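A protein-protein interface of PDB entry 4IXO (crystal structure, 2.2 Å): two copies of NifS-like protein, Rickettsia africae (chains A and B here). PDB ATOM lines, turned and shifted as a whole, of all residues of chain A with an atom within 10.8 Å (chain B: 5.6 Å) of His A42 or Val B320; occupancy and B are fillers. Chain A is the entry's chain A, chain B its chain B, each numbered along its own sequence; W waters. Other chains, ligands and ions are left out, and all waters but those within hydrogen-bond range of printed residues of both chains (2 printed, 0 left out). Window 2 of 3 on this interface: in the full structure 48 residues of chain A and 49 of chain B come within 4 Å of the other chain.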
ATOM      1  N   LYS A  34     -27.704 -12.788 -19.263  1.00  0.00           N
ATOM      2  CA  LYS A  34     -27.468 -12.259 -17.915  1.00  0.00           C
ATOM      3  C   LYS A  34     -28.455 -12.767 -16.883  1.00  0.00           C
ATOM      4  O   LYS A  34     -29.582 -13.142 -17.208  1.00  0.00           O
ATOM      5  CB  LYS A  34     -27.529 -10.735 -17.936  1.00  0.00           C
ATOM      6  CG  LYS A  34     -26.413 -10.086 -18.736  1.00  0.00           C
ATOM      7  CD  LYS A  34     -26.718  -8.619 -18.921  1.00  0.00           C
ATOM      8  CE  LYS A  34     -25.634  -7.887 -19.700  1.00  0.00           C
ATOM      9  NZ  LYS A  34     -24.342  -7.876 -18.977  1.00  0.00           N
ATOM     10  N   GLU A  35     -28.005 -12.768 -15.635  1.00  0.00           N
ATOM     11  CA  GLU A  35     -28.881 -12.922 -14.484  1.00  0.00           C
ATOM     12  C   GLU A  35     -29.338 -11.523 -14.107  1.00  0.00           C
ATOM     13  O   GLU A  35     -28.508 -10.647 -13.855  1.00  0.00           O
ATOM     14  CB  GLU A  35     -28.134 -13.565 -13.321  1.00  0.00           C
ATOM     15  CG  GLU A  35     -27.664 -14.986 -13.641  1.00  0.00           C
ATOM     16  CD  GLU A  35     -26.236 -15.090 -14.192  1.00  0.00           C
ATOM     17  OE1 GLU A  35     -25.530 -14.065 -14.295  1.00  0.00           O
ATOM     18  OE2 GLU A  35     -25.807 -16.227 -14.513  1.00  0.00           O
ATOM     19  N   LEU A  36     -30.643 -11.320 -14.030  1.00  0.00           N
ATOM     20  CA  LEU A  36     -31.196  -9.986 -13.823  1.00  0.00           C
ATOM     21  C   LEU A  36     -32.214  -9.972 -12.680  1.00  0.00           C
ATOM     22  O   LEU A  36     -33.393 -10.172 -12.909  1.00  0.00           O
ATOM     23  CB  LEU A  36     -31.844  -9.502 -15.126  1.00  0.00           C
ATOM     24  CG  LEU A  36     -30.929  -9.443 -16.367  1.00  0.00           C
ATOM     25  CD1 LEU A  36     -31.709  -9.333 -17.676  1.00  0.00           C
ATOM     26  CD2 LEU A  36     -29.973  -8.289 -16.241  1.00  0.00           C
ATOM     27  N   ASN A  37     -31.759  -9.726 -11.457  1.00  0.00           N
ATOM     28  CA  ASN A  37     -32.695  -9.479 -10.352  1.00  0.00           C
ATOM     29  C   ASN A  37     -32.349  -8.161  -9.656  1.00  0.00           C
ATOM     30  O   ASN A  37     -31.408  -8.089  -8.877  1.00  0.00           O
ATOM     31  CB  ASN A  37     -32.746 -10.624  -9.318  1.00  0.00           C
ATOM     32  CG  ASN A  37     -33.919 -10.469  -8.321  1.00  0.00           C
ATOM     33  OD1 ASN A  37     -34.317  -9.353  -8.007  1.00  0.00           O
ATOM     34  ND2 ASN A  37     -34.509 -11.603  -7.874  1.00  0.00           N
ATOM     35  N   PRO A  38     -33.135  -7.127  -9.926  1.00  0.00           N
ATOM     36  CA  PRO A  38     -32.899  -5.814  -9.358  1.00  0.00           C
ATOM     37  C   PRO A  38     -32.844  -5.777  -7.821  1.00  0.00           C
ATOM     38  O   PRO A  38     -32.244  -4.856  -7.289  1.00  0.00           O
ATOM     39  CB  PRO A  38     -34.091  -5.006  -9.859  1.00  0.00           C
ATOM     40  CG  PRO A  38     -34.457  -5.655 -11.136  1.00  0.00           C
ATOM     41  CD  PRO A  38     -34.261  -7.117 -10.867  1.00  0.00           C
ATOM     42  N   SER A  39     -33.455  -6.753  -7.137  1.00  0.00           N
ATOM     43  CA  SER A  39     -33.434  -6.797  -5.676  1.00  0.00           C
ATOM     44  C   SER A  39     -32.103  -7.295  -5.117  1.00  0.00           C
ATOM     45  O   SER A  39     -31.817  -7.074  -3.945  1.00  0.00           O
ATOM     46  CB  SER A  39     -34.607  -7.637  -5.103  1.00  0.00           C
ATOM     47  OG  SER A  39     -35.881  -7.098  -5.464  1.00  0.00           O
ATOM     48  N   SER A  40     -31.274  -7.930  -5.939  1.00  0.00           N
ATOM     49  CA  SER A  40     -29.989  -8.451  -5.455  1.00  0.00           C
ATOM     50  C   SER A  40     -28.967  -7.320  -5.267  1.00  0.00           C
ATOM     51  O   SER A  40     -28.856  -6.424  -6.118  1.00  0.00           O
ATOM     52  CB  SER A  40     -29.441  -9.539  -6.414  1.00  0.00           C
ATOM     53  OG  SER A  40     -30.305 -10.678  -6.523  1.00  0.00           O
ATOM     54  N   ALA A  41     -28.229  -7.372  -4.159  1.00  0.00           N
ATOM     55  CA  ALA A  41     -27.266  -6.299  -3.764  1.00  0.00           C
ATOM     56  C   ALA A  41     -25.911  -6.295  -4.515  1.00  0.00           C
ATOM     57  O   ALA A  41     -25.199  -5.258  -4.556  1.00  0.00           O
ATOM     58  CB  ALA A  41     -27.017  -6.348  -2.262  1.00  0.00           C
ATOM     59  N   HIS A  42     -25.568  -7.440  -5.106  1.00  0.00           N
ATOM     60  CA  HIS A  42     -24.322  -7.603  -5.837  1.00  0.00           C
ATOM     61  C   HIS A  42     -24.335  -6.940  -7.232  1.00  0.00           C
ATOM     62  O   HIS A  42     -25.326  -6.317  -7.652  1.00  0.00           O
ATOM     63  CB  HIS A  42     -23.974  -9.100  -5.925  1.00  0.00           C
ATOM     64  CG  HIS A  42     -25.094  -9.954  -6.434  1.00  0.00           C
ATOM     65  ND1 HIS A  42     -25.708  -9.731  -7.650  1.00  0.00           N
ATOM     66  CD2 HIS A  42     -25.705 -11.036  -5.899  1.00  0.00           C
ATOM     67  CE1 HIS A  42     -26.649 -10.638  -7.842  1.00  0.00           C
ATOM     68  NE2 HIS A  42     -26.667 -11.441  -6.792  1.00  0.00           N
ATOM     69  N   SER A  43     -23.229  -7.078  -7.956  1.00  0.00           N
ATOM     70  CA  SER A  43     -23.045  -6.366  -9.219  1.00  0.00           C
ATOM     71  C   SER A  43     -24.048  -6.673 -10.292  1.00  0.00           C
ATOM     72  O   SER A  43     -24.418  -5.793 -11.055  1.00  0.00           O
ATOM     73  CB  SER A  43     -21.690  -6.708  -9.815  1.00  0.00           C
ATOM     74  OG  SER A  43     -20.682  -6.187  -9.020  1.00  0.00           O
ATOM     75  N   SER A  44     -24.436  -7.934 -10.397  1.00  0.00           N
ATOM     76  CA  SER A  44     -25.438  -8.309 -11.371  1.00  0.00           C
ATOM     77  C   SER A  44     -26.757  -7.636 -11.046  1.00  0.00           C
ATOM     78  O   SER A  44     -27.460  -7.196 -11.949  1.00  0.00           O
ATOM     79  CB  SER A  44     -25.629  -9.829 -11.431  1.00  0.00           C
ATOM     80  OG  SER A  44     -24.398 -10.458 -11.711  1.00  0.00           O
ATOM     81  N   GLY A  45     -27.113  -7.622  -9.761  1.00  0.00           N
ATOM     82  CA  GLY A  45     -28.382  -7.088  -9.340  1.00  0.00           C
ATOM     83  C   GLY A  45     -28.426  -5.590  -9.595  1.00  0.00           C
ATOM     84  O   GLY A  45     -29.455  -5.060 -10.004  1.00  0.00           O
ATOM     85  N   ARG A  46     -27.304  -4.925  -9.339  1.00  0.00           N
ATOM     86  CA  ARG A  46     -27.195  -3.476  -9.497  1.00  0.00           C
ATOM     87  C   ARG A  46     -27.262  -3.115 -10.961  1.00  0.00           C
ATOM     88  O   ARG A  46     -27.836  -2.099 -11.329  1.00  0.00           O
ATOM     89  CB  ARG A  46     -25.892  -2.943  -8.915  1.00  0.00           C
ATOM     90  CG  ARG A  46     -25.811  -2.978  -7.398  1.00  0.00           C
ATOM     91  CD  ARG A  46     -24.726  -2.036  -6.847  1.00  0.00           C
ATOM     92  NE  ARG A  46     -23.366  -2.306  -7.328  1.00  0.00           N
ATOM     93  CZ  ARG A  46     -22.595  -3.299  -6.888  1.00  0.00           C
ATOM     94  NH1 ARG A  46     -23.021  -4.153  -5.953  1.00  0.00           N
ATOM     95  NH2 ARG A  46     -21.390  -3.445  -7.388  1.00  0.00           N
ATOM     96  N   PHE A  47     -26.686  -3.958 -11.809  1.00  0.00           N
ATOM     97  CA  PHE A  47     -26.845  -3.765 -13.242  1.00  0.00           C
ATOM     98  C   PHE A  47     -28.330  -3.856 -13.652  1.00  0.00           C
ATOM     99  O   PHE A  47     -28.836  -3.006 -14.350  1.00  0.00           O
ATOM    100  CB  PHE A  47     -26.007  -4.786 -14.003  1.00  0.00           C
ATOM    101  CG  PHE A  47     -26.067  -4.607 -15.486  1.00  0.00           C
ATOM    102  CD1 PHE A  47     -27.048  -5.230 -16.225  1.00  0.00           C
ATOM    103  CD2 PHE A  47     -25.133  -3.806 -16.133  1.00  0.00           C
ATOM    104  CE1 PHE A  47     -27.109  -5.062 -17.597  1.00  0.00           C
ATOM    105  CE2 PHE A  47     -25.186  -3.615 -17.507  1.00  0.00           C
ATOM    106  CZ  PHE A  47     -26.180  -4.248 -18.240  1.00  0.00           C
ATOM    107  N   ALA A  48     -29.028  -4.883 -13.196  1.00  0.00           N
ATOM    108  CA  ALA A  48     -30.453  -5.022 -13.508  1.00  0.00           C
ATOM    109  C   ALA A  48     -31.268  -3.804 -13.017  1.00  0.00           C
ATOM    110  O   ALA A  48     -32.187  -3.343 -13.677  1.00  0.00           O
ATOM    111  CB  ALA A  48     -31.017  -6.327 -12.929  1.00  0.00           C
ATOM    112  N   LYS A  49     -30.944  -3.341 -11.825  1.00  0.00           N
ATOM    113  CA  LYS A  49     -31.664  -2.223 -11.206  1.00  0.00           C
ATOM    114  C   LYS A  49     -31.445  -0.958 -12.049  1.00  0.00           C
ATOM    115  O   LYS A  49     -32.385  -0.252 -12.353  1.00  0.00           O
ATOM    116  CB  LYS A  49     -31.159  -2.024  -9.765  1.00  0.00           C
ATOM    117  CG  LYS A  49     -31.602  -0.736  -9.070  1.00  0.00           C
ATOM    118  CD  LYS A  49     -33.095  -0.807  -8.752  1.00  0.00           C
ATOM    119  CE  LYS A  49     -33.500   0.293  -7.791  1.00  0.00           C
ATOM    120  NZ  LYS A  49     -34.971   0.309  -7.690  1.00  0.00           N
ATOM    121  N   ASN A  50     -30.190  -0.701 -12.418  1.00  0.00           N
ATOM    122  CA  ASN A  50     -29.876   0.407 -13.300  1.00  0.00           C
ATOM    123  C   ASN A  50     -30.618   0.352 -14.622  1.00  0.00           C
ATOM    124  O   ASN A  50     -31.113   1.379 -15.062  1.00  0.00           O
ATOM    125  CB  ASN A  50     -28.376   0.570 -13.516  1.00  0.00           C
ATOM    126  CG  ASN A  50     -28.016   1.908 -14.199  1.00  0.00           C
ATOM    127  OD1 ASN A  50     -28.165   2.971 -13.610  1.00  0.00           O
ATOM    128  ND2 ASN A  50     -27.540   1.848 -15.430  1.00  0.00           N
ATOM    129  N   TYR B  11     -21.228 -16.746 -10.487  1.00  0.00           N
ATOM    130  CA  TYR B  11     -22.591 -16.570 -10.008  1.00  0.00           C
ATOM    131  C   TYR B  11     -23.081 -17.814  -9.261  1.00  0.00           C
ATOM    132  O   TYR B  11     -23.228 -18.887  -9.819  1.00  0.00           O
ATOM    133  CB  TYR B  11     -23.530 -16.193 -11.162  1.00  0.00           C
ATOM    134  CG  TYR B  11     -24.936 -15.812 -10.743  1.00  0.00           C
ATOM    135  CD1 TYR B  11     -25.929 -16.774 -10.625  1.00  0.00           C
ATOM    136  CD2 TYR B  11     -25.290 -14.478 -10.511  1.00  0.00           C
ATOM    137  CE1 TYR B  11     -27.206 -16.433 -10.264  1.00  0.00           C
ATOM    138  CE2 TYR B  11     -26.577 -14.133 -10.145  1.00  0.00           C
ATOM    139  CZ  TYR B  11     -27.529 -15.123 -10.033  1.00  0.00           C
ATOM    140  OH  TYR B  11     -28.811 -14.818  -9.701  1.00  0.00           O
ATOM    141  N   LEU B  12     -23.340 -17.615  -7.976  1.00  0.00           N
ATOM    142  CA  LEU B  12     -23.740 -18.675  -7.052  1.00  0.00           C
ATOM    143  C   LEU B  12     -24.998 -18.260  -6.267  1.00  0.00           C
ATOM    144  O   LEU B  12     -25.098 -18.501  -5.077  1.00  0.00           O
ATOM    145  CB  LEU B  12     -22.590 -18.915  -6.087  1.00  0.00           C
ATOM    146  CG  LEU B  12     -21.351 -19.538  -6.699  1.00  0.00           C
ATOM    147  CD1 LEU B  12     -20.186 -19.441  -5.751  1.00  0.00           C
ATOM    148  CD2 LEU B  12     -21.593 -20.988  -7.080  1.00  0.00           C
ATOM    149  N   ASP B  13     -25.931 -17.622  -6.975  1.00  0.00           N
ATOM    150  CA  ASP B  13     -27.147 -17.061  -6.425  1.00  0.00           C
ATOM    151  C   ASP B  13     -28.350 -17.477  -7.283  1.00  0.00           C
ATOM    152  O   ASP B  13     -29.285 -16.694  -7.560  1.00  0.00           O
ATOM    153  CB  ASP B  13     -27.051 -15.529  -6.365  1.00  0.00           C
ATOM    154  CG  ASP B  13     -28.074 -14.920  -5.425  1.00  0.00           C
ATOM    155  OD1 ASP B  13     -28.457 -15.571  -4.431  1.00  0.00           O
ATOM    156  OD2 ASP B  13     -28.470 -13.771  -5.679  1.00  0.00           O
ATOM    157  N   LEU B 310     -20.677  -9.668   2.397  1.00  0.00           N
ATOM    158  CA  LEU B 310     -21.140  -9.659   1.012  1.00  0.00           C
ATOM    159  C   LEU B 310     -20.412  -8.579   0.169  1.00  0.00           C
ATOM    160  O   LEU B 310     -20.222  -8.745  -1.037  1.00  0.00           O
ATOM    161  CB  LEU B 310     -22.666  -9.486   0.969  1.00  0.00           C
ATOM    162  CG  LEU B 310     -23.479 -10.718   1.378  1.00  0.00           C
ATOM    163  CD1 LEU B 310     -24.933 -10.352   1.656  1.00  0.00           C
ATOM    164  CD2 LEU B 310     -23.392 -11.758   0.280  1.00  0.00           C
ATOM    165  N   PHE B 313     -17.487 -10.385  -0.872  1.00  0.00           N
ATOM    166  CA  PHE B 313     -17.693 -11.319  -1.960  1.00  0.00           C
ATOM    167  C   PHE B 313     -17.802 -10.577  -3.287  1.00  0.00           C
ATOM    168  O   PHE B 313     -17.300 -11.052  -4.314  1.00  0.00           O
ATOM    169  CB  PHE B 313     -18.923 -12.210  -1.743  1.00  0.00           C
ATOM    170  CG  PHE B 313     -18.674 -13.367  -0.812  1.00  0.00           C
ATOM    171  CD1 PHE B 313     -17.916 -14.458  -1.229  1.00  0.00           C
ATOM    172  CD2 PHE B 313     -19.196 -13.374   0.467  1.00  0.00           C
ATOM    173  CE1 PHE B 313     -17.673 -15.520  -0.373  1.00  0.00           C
ATOM    174  CE2 PHE B 313     -18.981 -14.448   1.310  1.00  0.00           C
ATOM    175  CZ  PHE B 313     -18.215 -15.515   0.894  1.00  0.00           C
ATOM    176  N   ASP B 314     -18.459  -9.423  -3.256  1.00  0.00           N
ATOM    177  CA  ASP B 314     -18.662  -8.655  -4.469  1.00  0.00           C
ATOM    178  C   ASP B 314     -17.315  -8.151  -5.021  1.00  0.00           C
ATOM    179  O   ASP B 314     -17.089  -8.190  -6.215  1.00  0.00           O
ATOM    180  CB  ASP B 314     -19.596  -7.473  -4.229  1.00  0.00           C
ATOM    181  CG  ASP B 314     -20.139  -6.910  -5.523  1.00  0.00           C
ATOM    182  OD1 ASP B 314     -20.449  -7.704  -6.451  1.00  0.00           O
ATOM    183  OD2 ASP B 314     -20.277  -5.696  -5.607  1.00  0.00           O
ATOM    184  N   ILE B 318     -17.838 -12.450  -6.760  1.00  0.00           N
ATOM    185  CA  ILE B 318     -18.697 -13.592  -6.448  1.00  0.00           C
ATOM    186  C   ILE B 318     -20.091 -13.058  -6.100  1.00  0.00           C
ATOM    187  O   ILE B 318     -20.214 -12.157  -5.250  1.00  0.00           O
ATOM    188  CB  ILE B 318     -18.204 -14.398  -5.230  1.00  0.00           C
ATOM    189  CG1 ILE B 318     -16.697 -14.708  -5.282  1.00  0.00           C
ATOM    190  CG2 ILE B 318     -19.026 -15.659  -5.061  1.00  0.00           C
ATOM    191  CD1 ILE B 318     -16.296 -16.019  -5.905  1.00  0.00           C
ATOM    192  N   CYS B 319     -21.113 -13.606  -6.757  1.00  0.00           N
ATOM    193  CA  CYS B 319     -22.507 -13.291  -6.437  1.00  0.00           C
ATOM    194  C   CYS B 319     -23.100 -14.376  -5.546  1.00  0.00           C
ATOM    195  O   CYS B 319     -23.353 -15.523  -5.989  1.00  0.00           O
ATOM    196  CB  CYS B 319     -23.376 -13.120  -7.693  1.00  0.00           C
ATOM    197  SG  CYS B 319     -22.841 -11.733  -8.701  1.00  0.00           S
ATOM    198  N   VAL B 320     -23.286 -14.011  -4.283  1.00  0.00           N
ATOM    199  CA  VAL B 320     -24.073 -14.833  -3.352  1.00  0.00           C
ATOM    200  C   VAL B 320     -25.022 -13.881  -2.676  1.00  0.00           C
ATOM    201  O   VAL B 320     -25.083 -12.730  -3.073  1.00  0.00           O
ATOM    202  CB  VAL B 320     -23.192 -15.608  -2.346  1.00  0.00           C
ATOM    203  CG1 VAL B 320     -22.451 -16.717  -3.066  1.00  0.00           C
ATOM    204  CG2 VAL B 320     -22.218 -14.692  -1.623  1.00  0.00           C
ATOM    205  N   SER B 321     -25.768 -14.347  -1.675  1.00  0.00           N
ATOM    206  CA  SER B 321     -26.711 -13.490  -0.973  1.00  0.00           C
ATOM    207  C   SER B 321     -26.802 -13.880   0.493  1.00  0.00           C
ATOM    208  O   SER B 321     -26.114 -14.795   0.968  1.00  0.00           O
ATOM    209  CB  SER B 321     -28.107 -13.578  -1.628  1.00  0.00           C
ATOM    210  OG  SER B 321     -28.709 -14.855  -1.411  1.00  0.00           O
ATOM    211  N   SER B 322     -27.655 -13.168   1.204  1.00  0.00           N
ATOM    212  CA  SER B 322     -27.942 -13.449   2.578  1.00  0.00           C
ATOM    213  C   SER B 322     -29.317 -14.083   2.734  1.00  0.00           C
ATOM    214  O   SER B 322     -30.052 -14.302   1.750  1.00  0.00           O
ATOM    215  CB  SER B 322     -27.823 -12.166   3.384  1.00  0.00           C
ATOM    216  OG  SER B 322     -27.765 -12.475   4.756  1.00  0.00           O
ATOM    217  N   ILE B 351     -25.124 -16.567   4.950  1.00  0.00           N
ATOM    218  CA  ILE B 351     -24.751 -16.511   3.547  1.00  0.00           C
ATOM    219  C   ILE B 351     -25.348 -17.713   2.834  1.00  0.00           C
ATOM    220  O   ILE B 351     -25.256 -18.838   3.341  1.00  0.00           O
ATOM    221  CB  ILE B 351     -23.228 -16.581   3.375  1.00  0.00           C
ATOM    222  CG1 ILE B 351     -22.537 -15.423   4.081  1.00  0.00           C
ATOM    223  CG2 ILE B 351     -22.876 -16.594   1.906  1.00  0.00           C
ATOM    224  CD1 ILE B 351     -22.779 -14.101   3.411  1.00  0.00           C
ATOM    225  N   ARG B 352     -26.021 -17.456   1.714  1.00  0.00           N
ATOM    226  CA  ARG B 352     -26.630 -18.490   0.875  1.00  0.00           C
ATOM    227  C   ARG B 352     -25.850 -18.658  -0.429  1.00  0.00           C
ATOM    228  O   ARG B 352     -25.670 -17.693  -1.198  1.00  0.00           O
ATOM    229  CB  ARG B 352     -28.077 -18.128   0.520  1.00  0.00           C
ATOM    230  CG  ARG B 352     -28.826 -19.273  -0.190  1.00  0.00           C
ATOM    231  CD  ARG B 352     -30.248 -18.884  -0.612  1.00  0.00           C
ATOM    232  NE  ARG B 352     -30.203 -17.905  -1.694  1.00  0.00           N
ATOM    233  CZ  ARG B 352     -31.223 -17.166  -2.096  1.00  0.00           C
ATOM    234  NH1 ARG B 352     -32.414 -17.294  -1.539  1.00  0.00           N
ATOM    235  NH2 ARG B 352     -31.062 -16.292  -3.079  1.00  0.00           N
ATOM    236  N   ILE B 353     -25.391 -19.889  -0.643  1.00  0.00           N
ATOM    237  CA  ILE B 353     -24.790 -20.316  -1.874  1.00  0.00           C
ATOM    238  C   ILE B 353     -25.765 -21.249  -2.570  1.00  0.00           C
ATOM    239  O   ILE B 353     -26.123 -22.288  -2.036  1.00  0.00           O
ATOM    240  CB  ILE B 353     -23.467 -21.029  -1.617  1.00  0.00           C
ATOM    241  CG1 ILE B 353     -22.555 -20.143  -0.788  1.00  0.00           C
ATOM    242  CG2 ILE B 353     -22.764 -21.355  -2.912  1.00  0.00           C
ATOM    243  CD1 ILE B 353     -22.540 -20.542   0.673  1.00  0.00           C
ATOM    244  N   PHE B 367     -15.120 -19.816  -4.902  1.00  0.00           N
ATOM    245  CA  PHE B 367     -15.852 -19.380  -3.745  1.00  0.00           C
ATOM    246  C   PHE B 367     -15.032 -19.584  -2.458  1.00  0.00           C
ATOM    247  O   PHE B 367     -14.962 -18.699  -1.618  1.00  0.00           O
ATOM    248  CB  PHE B 367     -17.192 -20.107  -3.643  1.00  0.00           C
ATOM    249  CG  PHE B 367     -17.917 -19.813  -2.380  1.00  0.00           C
ATOM    250  CD1 PHE B 367     -18.697 -18.676  -2.263  1.00  0.00           C
ATOM    251  CD2 PHE B 367     -17.753 -20.633  -1.273  1.00  0.00           C
ATOM    252  CE1 PHE B 367     -19.333 -18.387  -1.083  1.00  0.00           C
ATOM    253  CE2 PHE B 367     -18.369 -20.322  -0.088  1.00  0.00           C
ATOM    254  CZ  PHE B 367     -19.175 -19.214  -0.004  1.00  0.00           C
HETATM  255  O   HOH W   1     -30.113 -12.163  -4.211  1.00  0.00           O
HETATM  256  O   HOH W   2     -29.359 -12.455  -8.577  1.00  0.00           O
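The side-chain carboxylate (OD2) of Asp B314 lies within salt-bridge range of the guanidinium group (NH2) of Arg A46 (3.1 Å). NE2 of His A42 lies within hydrogen-bond range of OD2 of Asp B13 (3.1 Å). The side-chain hydroxyl of Ser A43 lies within hydrogen-bond range of the side-chain carboxylate of Asp B314. A ring nitrogen (ND1) of His A42 lies within hydrogen-bond range of the side-chain sulfur of Cys B319 (3.7 Å). SG of Cys B319 sits at hydrogen-bond distance from OG of Ser A44, at 3.6 Å.
The guanidinium group (NH2) of Arg A46 is in hydrogen-bond range of the side-chain hydroxyl (OG) of Ser A43 (3.3 Å). The backbone carbonyl oxygen (O) of Ala A41 is in hydrogen-bond range of the guanidinium group (NH1) of Arg A46, 2.8 Å away. The side-chain hydroxyl (OG) of Ser B321 sits at hydrogen-bond distance from the side-chain carboxylate (OD1) of Asp B13 (3.1 Å). The backbone carbonyl oxygen (O) of Asp B13 sits at hydrogen-bond distance from the side-chain hydroxyl (OH) of Tyr B11, at 2.9 Å. N of Gly A45 is in hydrogen-bond range of ND1 of His A42, 3.3 Å away. OD1 of Asp B13 lies within salt-bridge range of NH2 of Arg B352 (3.0 Å).
Among the printed residues, merely in contact across the chains: His A42 with Val B320 (3.4 Å), Glu A35 with Tyr B11 (3.6 Å), Ser A40 with Asp B13 (3.7 Å) and His A42 with Asp B314 (3.8 Å).
His A42 touches just these residues of chain B: Asp B13, Asp B314, Cys B319 and Val B320. Val B320 touches just one residue of chain A: His A42 (3.4 Å). Cys B319 touches just these residues of chain A: His A42 and Ser A44. No residue of chain A comes within 4 Å of Ser B321. Of the printed residues of chain A, Tyr B11 touches Glu A35 (3.6 Å). Printed residues of chain B within 4 Å of Ser A40: Asp B13 (3.7 Å). Of the printed residues of chain B, Arg A46 touches Asp B314 (3.1 Å). Printed residues of chain A within 4 Å of Asp B314: His A42, Ser A43 and Arg A46. Asn A50 touches none of the printed residues of chain B.
Of the 17 printed residues of chain A, 6 touch a printed residue of chain B. Hydrophobic or aromatic side chains of chain A within 4 Å of the printed part of chain B: His A42. Printed residues of chain B that touch a printed residue of chain A: Tyr B11, Asp B13, Asp B314, Cys B319 and Val B320. Hydrophobic or aromatic side chains of chain B within 4 Å of the printed part of chain A: Tyr B11. Among the printed residues, 9 pairs touch across the chains.
No position is printed for both chains.
Water W2 lies within hydrogen-bond range of OH of Tyr B11, OG of Ser A40, OD2 of Asp B13 and NE2 of His A42. Water W1 bridges the side-chain carboxylate of Asp B13 and the side-chain hydroxyl of Ser A40.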
